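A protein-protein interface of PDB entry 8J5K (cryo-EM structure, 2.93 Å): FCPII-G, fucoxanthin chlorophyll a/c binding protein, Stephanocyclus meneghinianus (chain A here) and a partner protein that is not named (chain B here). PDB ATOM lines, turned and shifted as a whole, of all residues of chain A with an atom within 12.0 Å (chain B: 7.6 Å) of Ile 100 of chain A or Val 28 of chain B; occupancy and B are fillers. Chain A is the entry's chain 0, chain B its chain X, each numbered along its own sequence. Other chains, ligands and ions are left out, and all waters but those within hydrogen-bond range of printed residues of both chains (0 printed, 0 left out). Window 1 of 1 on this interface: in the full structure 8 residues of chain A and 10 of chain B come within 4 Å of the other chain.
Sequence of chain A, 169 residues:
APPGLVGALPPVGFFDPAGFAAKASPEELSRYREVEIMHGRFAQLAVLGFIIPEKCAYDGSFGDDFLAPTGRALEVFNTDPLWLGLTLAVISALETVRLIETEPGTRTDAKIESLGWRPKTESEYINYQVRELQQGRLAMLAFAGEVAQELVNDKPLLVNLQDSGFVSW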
ATOM      1  N   VAL A  90      17.775  -9.819  -1.984  1.00  0.00           N
ATOM      2  CA  VAL A  90      19.116  -9.533  -1.467  1.00  0.00           C
ATOM      3  C   VAL A  90      19.135  -8.184  -0.758  1.00  0.00           C
ATOM      4  O   VAL A  90      19.735  -8.032   0.320  1.00  0.00           O
ATOM      5  CB  VAL A  90      20.152  -9.590  -2.604  1.00  0.00           C
ATOM      6  CG1 VAL A  90      21.492  -9.059  -2.126  1.00  0.00           C
ATOM      7  CG2 VAL A  90      20.295 -11.009  -3.118  1.00  0.00           C
ATOM      8  N   ILE A  91      18.487  -7.182  -1.358  1.00  0.00           N
ATOM      9  CA  ILE A  91      18.362  -5.882  -0.706  1.00  0.00           C
ATOM     10  C   ILE A  91      17.690  -6.039   0.650  1.00  0.00           C
ATOM     11  O   ILE A  91      18.129  -5.460   1.651  1.00  0.00           O
ATOM     12  CB  ILE A  91      17.585  -4.906  -1.607  1.00  0.00           C
ATOM     13  CG1 ILE A  91      18.461  -4.414  -2.755  1.00  0.00           C
ATOM     14  CG2 ILE A  91      17.068  -3.730  -0.798  1.00  0.00           C
ATOM     15  CD1 ILE A  91      17.755  -3.444  -3.668  1.00  0.00           C
ATOM     16  N   SER A  92      16.621  -6.837   0.701  1.00  0.00           N
ATOM     17  CA  SER A  92      15.899  -7.049   1.947  1.00  0.00           C
ATOM     18  C   SER A  92      16.784  -7.700   2.999  1.00  0.00           C
ATOM     19  O   SER A  92      16.698  -7.364   4.180  1.00  0.00           O
ATOM     20  CB  SER A  92      14.671  -7.917   1.691  1.00  0.00           C
ATOM     21  OG  SER A  92      15.063  -9.219   1.297  1.00  0.00           O
ATOM     22  N   ALA A  93      17.620  -8.653   2.592  1.00  0.00           N
ATOM     23  CA  ALA A  93      18.497  -9.320   3.552  1.00  0.00           C
ATOM     24  C   ALA A  93      19.514  -8.347   4.142  1.00  0.00           C
ATOM     25  O   ALA A  93      19.692  -8.279   5.367  1.00  0.00           O
ATOM     26  CB  ALA A  93      19.204 -10.501   2.887  1.00  0.00           C
ATOM     27  N   LEU A  94      20.187  -7.580   3.281  1.00  0.00           N
ATOM     28  CA  LEU A  94      21.154  -6.613   3.796  1.00  0.00           C
ATOM     29  C   LEU A  94      20.471  -5.554   4.658  1.00  0.00           C
ATOM     30  O   LEU A  94      21.040  -5.086   5.657  1.00  0.00           O
ATOM     31  CB  LEU A  94      21.924  -5.978   2.640  1.00  0.00           C
ATOM     32  CG  LEU A  94      22.620  -6.993   1.729  1.00  0.00           C
ATOM     33  CD1 LEU A  94      23.478  -6.300   0.687  1.00  0.00           C
ATOM     34  CD2 LEU A  94      23.456  -7.968   2.545  1.00  0.00           C
ATOM     35  N   GLU A  95      19.231  -5.197   4.333  1.00  0.00           N
ATOM     36  CA  GLU A  95      18.535  -4.232   5.166  1.00  0.00           C
ATOM     37  C   GLU A  95      18.032  -4.842   6.468  1.00  0.00           C
ATOM     38  O   GLU A  95      17.863  -4.124   7.456  1.00  0.00           O
ATOM     39  CB  GLU A  95      17.377  -3.603   4.403  1.00  0.00           C
ATOM     40  CG  GLU A  95      16.846  -2.389   5.111  1.00  0.00           C
ATOM     41  CD  GLU A  95      16.137  -1.459   4.179  1.00  0.00           C
ATOM     42  OE1 GLU A  95      15.847  -1.876   3.041  1.00  0.00           O
ATOM     43  OE2 GLU A  95      15.889  -0.305   4.577  1.00  0.00           O
ATOM     44  N   THR A  96      17.765  -6.146   6.495  1.00  0.00           N
ATOM     45  CA  THR A  96      17.499  -6.794   7.772  1.00  0.00           C
ATOM     46  C   THR A  96      18.742  -6.760   8.644  1.00  0.00           C
ATOM     47  O   THR A  96      18.652  -6.575   9.862  1.00  0.00           O
ATOM     48  CB  THR A  96      17.024  -8.230   7.563  1.00  0.00           C
ATOM     49  OG1 THR A  96      15.822  -8.226   6.788  1.00  0.00           O
ATOM     50  CG2 THR A  96      16.743  -8.892   8.904  1.00  0.00           C
ATOM     51  N   VAL A  97      19.916  -6.926   8.028  1.00  0.00           N
ATOM     52  CA  VAL A  97      21.160  -6.704   8.763  1.00  0.00           C
ATOM     53  C   VAL A  97      21.181  -5.298   9.349  1.00  0.00           C
ATOM     54  O   VAL A  97      21.538  -5.100  10.519  1.00  0.00           O
ATOM     55  CB  VAL A  97      22.377  -6.953   7.854  1.00  0.00           C
ATOM     56  CG1 VAL A  97      23.657  -6.605   8.589  1.00  0.00           C
ATOM     57  CG2 VAL A  97      22.404  -8.399   7.399  1.00  0.00           C
ATOM     58  N   ARG A  98      20.793  -4.303   8.548  1.00  0.00           N
ATOM     59  CA  ARG A  98      20.664  -2.943   9.070  1.00  0.00           C
ATOM     60  C   ARG A  98      19.745  -2.899  10.289  1.00  0.00           C
ATOM     61  O   ARG A  98      20.160  -2.504  11.383  1.00  0.00           O
ATOM     62  CB  ARG A  98      20.149  -1.994   7.985  1.00  0.00           C
ATOM     63  CG  ARG A  98      20.389  -0.526   8.305  1.00  0.00           C
ATOM     64  CD  ARG A  98      20.250   0.357   7.079  1.00  0.00           C
ATOM     65  NE  ARG A  98      18.883   0.389   6.574  1.00  0.00           N
ATOM     66  CZ  ARG A  98      17.973   1.282   6.933  1.00  0.00           C
ATOM     67  NH1 ARG A  98      18.250   2.243   7.798  1.00  0.00           N
ATOM     68  NH2 ARG A  98      16.753   1.211   6.409  1.00  0.00           N
ATOM     69  N   LEU A  99      18.490  -3.328  10.113  1.00  0.00           N
ATOM     70  CA  LEU A  99      17.503  -3.277  11.192  1.00  0.00           C
ATOM     71  C   LEU A  99      18.005  -3.960  12.454  1.00  0.00           C
ATOM     72  O   LEU A  99      17.708  -3.508  13.567  1.00  0.00           O
ATOM     73  CB  LEU A  99      16.190  -3.930  10.748  1.00  0.00           C
ATOM     74  CG  LEU A  99      15.196  -4.233  11.876  1.00  0.00           C
ATOM     75  CD1 LEU A  99      14.618  -2.951  12.455  1.00  0.00           C
ATOM     76  CD2 LEU A  99      14.088  -5.172  11.426  1.00  0.00           C
ATOM     77  N   ILE A 100      18.770  -5.039  12.307  1.00  0.00           N
ATOM     78  CA  ILE A 100      19.296  -5.729  13.478  1.00  0.00           C
ATOM     79  C   ILE A 100      20.372  -4.889  14.152  1.00  0.00           C
ATOM     80  O   ILE A 100      20.305  -4.624  15.356  1.00  0.00           O
ATOM     81  CB  ILE A 100      19.829  -7.120  13.096  1.00  0.00           C
ATOM     82  CG1 ILE A 100      18.703  -7.999  12.562  1.00  0.00           C
ATOM     83  CG2 ILE A 100      20.457  -7.787  14.299  1.00  0.00           C
ATOM     84  CD1 ILE A 100      19.195  -9.278  11.927  1.00  0.00           C
ATOM     85  N   GLU A 101      21.379  -4.449  13.394  1.00  0.00           N
ATOM     86  CA  GLU A 101      22.500  -3.773  14.039  1.00  0.00           C
ATOM     87  C   GLU A 101      22.165  -2.365  14.503  1.00  0.00           C
ATOM     88  O   GLU A 101      22.012  -2.149  15.710  1.00  0.00           O
ATOM     89  CB  GLU A 101      23.710  -3.718  13.111  1.00  0.00           C
ATOM     90  CG  GLU A 101      24.063  -5.034  12.476  1.00  0.00           C
ATOM     91  CD  GLU A 101      24.745  -5.971  13.446  1.00  0.00           C
ATOM     92  OE1 GLU A 101      25.987  -5.934  13.522  1.00  0.00           O
ATOM     93  OE2 GLU A 101      24.040  -6.734  14.138  1.00  0.00           O
ATOM     94  N   THR A 102      21.972  -1.432  13.562  1.00  0.00           N
ATOM     95  CA  THR A 102      21.662  -0.038  13.881  1.00  0.00           C
ATOM     96  C   THR A 102      20.582   0.029  14.960  1.00  0.00           C
ATOM     97  O   THR A 102      19.694  -0.837  14.986  1.00  0.00           O
ATOM     98  CB  THR A 102      21.197   0.706  12.611  1.00  0.00           C
ATOM     99  OG1 THR A 102      20.013   0.078  12.095  1.00  0.00           O
ATOM    100  CG2 THR A 102      22.272   0.688  11.504  1.00  0.00           C
ATOM    101  N   GLU A 103      20.593   1.017  15.852  1.00  0.00           N
ATOM    102  CA  GLU A 103      19.595   1.142  16.914  1.00  0.00           C
ATOM    103  C   GLU A 103      18.708   2.362  16.690  1.00  0.00           C
ATOM    104  O   GLU A 103      19.127   3.310  16.014  1.00  0.00           O
ATOM    105  CB  GLU A 103      20.254   1.262  18.293  1.00  0.00           C
ATOM    106  N   PRO A 104      17.492   2.400  17.271  1.00  0.00           N
ATOM    107  CA  PRO A 104      16.576   3.513  16.970  1.00  0.00           C
ATOM    108  C   PRO A 104      17.260   4.845  17.206  1.00  0.00           C
ATOM    109  O   PRO A 104      17.933   5.043  18.217  1.00  0.00           O
ATOM    110  CB  PRO A 104      15.422   3.314  17.956  1.00  0.00           C
ATOM    111  CG  PRO A 104      15.367   1.873  18.175  1.00  0.00           C
ATOM    112  CD  PRO A 104      16.814   1.386  18.112  1.00  0.00           C
ATOM    113  N   GLY A 105      17.099   5.761  16.261  1.00  0.00           N
ATOM    114  CA  GLY A 105      17.860   6.990  16.334  1.00  0.00           C
ATOM    115  C   GLY A 105      19.026   7.007  15.371  1.00  0.00           C
ATOM    116  O   GLY A 105      19.315   8.057  14.799  1.00  0.00           O
ATOM    117  N   THR A 106      19.734   5.889  15.191  1.00  0.00           N
ATOM    118  CA  THR A 106      20.777   5.921  14.175  1.00  0.00           C
ATOM    119  C   THR A 106      20.245   5.578  12.788  1.00  0.00           C
ATOM    120  O   THR A 106      19.714   6.463  12.104  1.00  0.00           O
ATOM    121  CB  THR A 106      21.880   4.932  14.543  1.00  0.00           C
ATOM    122  OG1 THR A 106      21.317   3.623  14.639  1.00  0.00           O
ATOM    123  CG2 THR A 106      22.507   5.305  15.876  1.00  0.00           C
ATOM    124  N   ARG A 107      20.297   4.313  12.407  1.00  0.00           N
ATOM    125  CA  ARG A 107      19.699   3.885  11.144  1.00  0.00           C
ATOM    126  C   ARG A 107      20.186   4.671   9.965  1.00  0.00           C
ATOM    127  O   ARG A 107      19.518   4.733   8.952  1.00  0.00           O
ATOM    128  CB  ARG A 107      18.176   3.982  11.214  1.00  0.00           C
ATOM    129  CG  ARG A 107      17.455   2.736  11.680  1.00  0.00           C
ATOM    130  CD  ARG A 107      17.487   2.609  13.188  1.00  0.00           C
ATOM    131  NE  ARG A 107      16.372   1.807  13.671  1.00  0.00           N
ATOM    132  CZ  ARG A 107      16.380   0.483  13.722  1.00  0.00           C
ATOM    133  NH1 ARG A 107      17.443  -0.189  13.313  1.00  0.00           N
ATOM    134  NH2 ARG A 107      15.322  -0.167  14.177  1.00  0.00           N
ATOM    135  N   THR A 108      21.338   5.286  10.081  1.00  0.00           N
ATOM    136  CA  THR A 108      21.906   5.972   8.918  1.00  0.00           C
ATOM    137  C   THR A 108      23.432   5.908   8.916  1.00  0.00           C
ATOM    138  O   THR A 108      24.070   5.967   7.855  1.00  0.00           O
ATOM    139  CB  THR A 108      21.384   7.413   8.872  1.00  0.00           C
ATOM    140  OG1 THR A 108      19.990   7.378   8.548  1.00  0.00           O
ATOM    141  CG2 THR A 108      22.115   8.258   7.850  1.00  0.00           C
ATOM    142  N   ASP A 109      24.018   5.752  10.104  1.00  0.00           N
ATOM    143  CA  ASP A 109      25.468   5.688  10.261  1.00  0.00           C
ATOM    144  C   ASP A 109      25.880   4.241  10.044  1.00  0.00           C
ATOM    145  O   ASP A 109      25.702   3.394  10.921  1.00  0.00           O
ATOM    146  CB  ASP A 109      25.875   6.190  11.642  1.00  0.00           C
ATOM    147  CG  ASP A 109      27.384   6.180  11.861  1.00  0.00           C
ATOM    148  OD1 ASP A 109      28.123   5.588  11.046  1.00  0.00           O
ATOM    149  OD2 ASP A 109      27.836   6.766  12.865  1.00  0.00           O
ATOM    150  N   ALA A 110      26.437   3.957   8.874  1.00  0.00           N
ATOM    151  CA  ALA A 110      26.926   2.624   8.567  1.00  0.00           C
ATOM    152  C   ALA A 110      28.297   2.358   9.162  1.00  0.00           C
ATOM    153  O   ALA A 110      28.920   1.351   8.811  1.00  0.00           O
ATOM    154  CB  ALA A 110      26.969   2.412   7.053  1.00  0.00           C
ATOM    155  N   LYS A 111      28.783   3.240  10.041  1.00  0.00           N
ATOM    156  CA  LYS A 111      30.109   3.109  10.638  1.00  0.00           C
ATOM    157  C   LYS A 111      31.179   2.955   9.564  1.00  0.00           C
ATOM    158  O   LYS A 111      32.208   2.312   9.776  1.00  0.00           O
ATOM    159  CB  LYS A 111      30.156   1.944  11.629  1.00  0.00           C
ATOM    160  CG  LYS A 111      28.965   1.895  12.575  1.00  0.00           C
ATOM    161  CD  LYS A 111      29.288   2.525  13.919  1.00  0.00           C
ATOM    162  CE  LYS A 111      28.039   2.680  14.775  1.00  0.00           C
ATOM    163  NZ  LYS A 111      27.159   1.482  14.719  1.00  0.00           N
ATOM    164  N   ILE B  22      21.894 -17.009   5.549  1.00  0.00           N
ATOM    165  CA  ILE B  22      22.654 -17.770   6.539  1.00  0.00           C
ATOM    166  C   ILE B  22      23.331 -16.825   7.526  1.00  0.00           C
ATOM    167  O   ILE B  22      23.287 -17.036   8.747  1.00  0.00           O
ATOM    168  CB  ILE B  22      23.671 -18.697   5.849  1.00  0.00           C
ATOM    169  CG1 ILE B  22      22.974 -19.953   5.329  1.00  0.00           C
ATOM    170  CG2 ILE B  22      24.779 -19.084   6.812  1.00  0.00           C
ATOM    171  CD1 ILE B  22      23.866 -20.843   4.500  1.00  0.00           C
ATOM    172  N   ALA B  23      23.947 -15.754   7.016  1.00  0.00           N
ATOM    173  CA  ALA B  23      24.618 -14.797   7.889  1.00  0.00           C
ATOM    174  C   ALA B  23      23.632 -14.089   8.808  1.00  0.00           C
ATOM    175  O   ALA B  23      23.933 -13.850   9.982  1.00  0.00           O
ATOM    176  CB  ALA B  23      25.395 -13.780   7.054  1.00  0.00           C
ATOM    177  N   ILE B  24      22.459 -13.724   8.288  1.00  0.00           N
ATOM    178  CA  ILE B  24      21.456 -13.050   9.108  1.00  0.00           C
ATOM    179  C   ILE B  24      20.995 -13.963  10.233  1.00  0.00           C
ATOM    180  O   ILE B  24      20.843 -13.528  11.382  1.00  0.00           O
ATOM    181  CB  ILE B  24      20.276 -12.583   8.237  1.00  0.00           C
ATOM    182  N   ALA B  25      20.767 -15.241   9.923  1.00  0.00           N
ATOM    183  CA  ALA B  25      20.385 -16.190  10.963  1.00  0.00           C
ATOM    184  C   ALA B  25      21.476 -16.319  12.017  1.00  0.00           C
ATOM    185  O   ALA B  25      21.186 -16.346  13.221  1.00  0.00           O
ATOM    186  CB  ALA B  25      20.073 -17.550  10.344  1.00  0.00           C
ATOM    187  N   LEU B  26      22.739 -16.398  11.585  1.00  0.00           N
ATOM    188  CA  LEU B  26      23.834 -16.506  12.546  1.00  0.00           C
ATOM    189  C   LEU B  26      23.913 -15.274  13.438  1.00  0.00           C
ATOM    190  O   LEU B  26      24.095 -15.392  14.656  1.00  0.00           O
ATOM    191  CB  LEU B  26      25.160 -16.717  11.821  1.00  0.00           C
ATOM    192  CG  LEU B  26      25.431 -18.131  11.316  1.00  0.00           C
ATOM    193  CD1 LEU B  26      26.801 -18.202  10.672  1.00  0.00           C
ATOM    194  CD2 LEU B  26      25.323 -19.121  12.459  1.00  0.00           C
ATOM    195  N   ILE B  27      23.776 -14.085  12.852  1.00  0.00           N
ATOM    196  CA  ILE B  27      23.839 -12.860  13.642  1.00  0.00           C
ATOM    197  C   ILE B  27      22.697 -12.812  14.645  1.00  0.00           C
ATOM    198  O   ILE B  27      22.895 -12.455  15.811  1.00  0.00           O
ATOM    199  CB  ILE B  27      23.839 -11.623  12.726  1.00  0.00           C
ATOM    200  CG1 ILE B  27      25.083 -11.614  11.842  1.00  0.00           C
ATOM    201  CG2 ILE B  27      23.769 -10.351  13.549  1.00  0.00           C
ATOM    202  CD1 ILE B  27      25.034 -10.583  10.743  1.00  0.00           C
ATOM    203  N   VAL B  28      21.496 -13.182  14.245  1.00  0.00           N
ATOM    204  CA  VAL B  28      20.402 -13.081  15.187  1.00  0.00           C
ATOM    205  C   VAL B  28      20.675 -13.951  16.398  1.00  0.00           C
ATOM    206  O   VAL B  28      20.668 -13.468  17.526  1.00  0.00           O
ATOM    207  CB  VAL B  28      19.068 -13.499  14.566  1.00  0.00           C
ATOM    208  CG1 VAL B  28      18.037 -13.749  15.652  1.00  0.00           C
ATOM    209  CG2 VAL B  28      18.584 -12.435  13.597  1.00  0.00           C
ATOM    210  N   ILE B  29      20.938 -15.231  16.179  1.00  0.00           N
ATOM    211  CA  ILE B  29      21.144 -16.145  17.298  1.00  0.00           C
ATOM    212  C   ILE B  29      22.365 -15.781  18.127  1.00  0.00           C
ATOM    213  O   ILE B  29      22.249 -15.514  19.317  1.00  0.00           O
ATOM    214  CB  ILE B  29      21.263 -17.609  16.829  1.00  0.00           C
ATOM    215  CG1 ILE B  29      21.704 -18.499  17.989  1.00  0.00           C
ATOM    216  CG2 ILE B  29      22.232 -17.738  15.669  1.00  0.00           C
ATOM    217  CD1 ILE B  29      20.689 -18.584  19.107  1.00  0.00           C
ATOM    218  N   SER B  30      23.534 -15.758  17.511  1.00  0.00           N
ATOM    219  CA  SER B  30      24.757 -15.481  18.245  1.00  0.00           C
ATOM    220  C   SER B  30      24.607 -14.342  19.230  1.00  0.00           C
ATOM    221  O   SER B  30      25.178 -14.379  20.311  1.00  0.00           O
ATOM    222  CB  SER B  30      25.882 -15.156  17.276  1.00  0.00           C
ATOM    223  OG  SER B  30      27.027 -14.706  17.973  1.00  0.00           O
ATOM    224  N   LYS B  31      23.849 -13.324  18.862  1.00  0.00           N
ATOM    225  CA  LYS B  31      23.683 -12.179  19.737  1.00  0.00           C
ATOM    226  C   LYS B  31      22.716 -12.508  20.846  1.00  0.00           C
ATOM    227  O   LYS B  31      22.999 -12.257  22.013  1.00  0.00           O
ATOM    228  CB  LYS B  31      23.180 -10.976  18.952  1.00  0.00           C
ATOM    229  CG  LYS B  31      24.271  -9.988  18.586  1.00  0.00           C
ATOM    230  CD  LYS B  31      24.069  -9.448  17.183  1.00  0.00           C
ATOM    231  CE  LYS B  31      22.658  -8.918  17.001  1.00  0.00           C
ATOM    232  NZ  LYS B  31      22.622  -7.432  17.072  1.00  0.00           N
ATOM    233  N   SER B  32      21.576 -13.080  20.490  1.00  0.00           N
ATOM    234  CA  SER B  32      20.563 -13.410  21.481  1.00  0.00           C
ATOM    235  C   SER B  32      20.902 -14.692  22.196  1.00  0.00           C
ATOM    236  O   SER B  32      20.013 -15.472  22.522  1.00  0.00           O
ATOM    237  CB  SER B  32      19.203 -13.557  20.813  1.00  0.00           C
ATOM    238  OG  SER B  32      19.253 -14.515  19.771  1.00  0.00           O
ATOM    239  N   ASP B  33      22.183 -14.916  22.449  1.00  0.00           N
ATOM    240  CA  ASP B  33      22.608 -16.147  23.088  1.00  0.00           C
ATOM    241  C   ASP B  33      24.066 -16.029  23.445  1.00  0.00           C
ATOM    242  O   ASP B  33      24.848 -16.945  23.205  1.00  0.00           O
ATOM    243  CB  ASP B  33      22.395 -17.325  22.148  1.00  0.00           C
ATOM    244  CG  ASP B  33      22.637 -18.658  22.818  1.00  0.00           C
ATOM    245  OD1 ASP B  33      22.505 -18.732  24.056  1.00  0.00           O
ATOM    246  OD2 ASP B  33      22.962 -19.630  22.105  1.00  0.00           O
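Of chain B, only Val 28 and Lys 31 come within 4 Å of Ile 100 of chain A.
Of chain A, only Ile 100 (3.6 Å) comes within 4 Å of Val 28 of chain B.
No residue of chain A comes within 4 Å of Ala 25 of chain B.
Of chain A, only Glu 101 (3.7 Å) comes within 4 Å of Ile 27 of chain B.
No residue of chain A comes within 4 Å of Ile 29 of chain B.
Of the printed residues of chain A, Lys 31 of chain B touches Ile 100 and Glu 101.
Printed residues of chain B within 4 Å of Glu 101 of chain A: Ile 27 and Lys 31.
The nearest residue of chain B that does not touch Ile 100 of chain A is Ile 27 of chain B (4.3 Å).
The nearest residue of chain A that does not touch Val 28 of chain B is Thr 96 of chain A (6.2 Å).
Ile 100 of chain A touches Val 28 of chain B.
Ile 100 of chain A touches Lys 31 of chain B (CG2 to NZ, 3.5 Å).
Glu 101 of chain A touches Ile 27 of chain B (OE2 to CG2, 3.7 Å).
The side-chain hydroxyl (OG) of Ser 32 of chain B sits at hydrogen-bond distance from the backbone carbonyl oxygen (O) of Val 28 of chain B, 2.9 Å away.
Hydrophobic or aromatic side chains of chain A within 4 Å of the printed part of chain B: Ile 100.
Among the printed residues, 4 pairs touch across the chains.
Among the printed residues, Asp or Glu carboxylates within 4 Å of a Lys or Arg side-chain nitrogen of the other chain: Glu 101 of chain A with Lys 31 of chain B.
NZ of Lys 31 of chain B is in salt-bridge range of OE2 of Glu 101 of chain A, 3.3 Å away.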
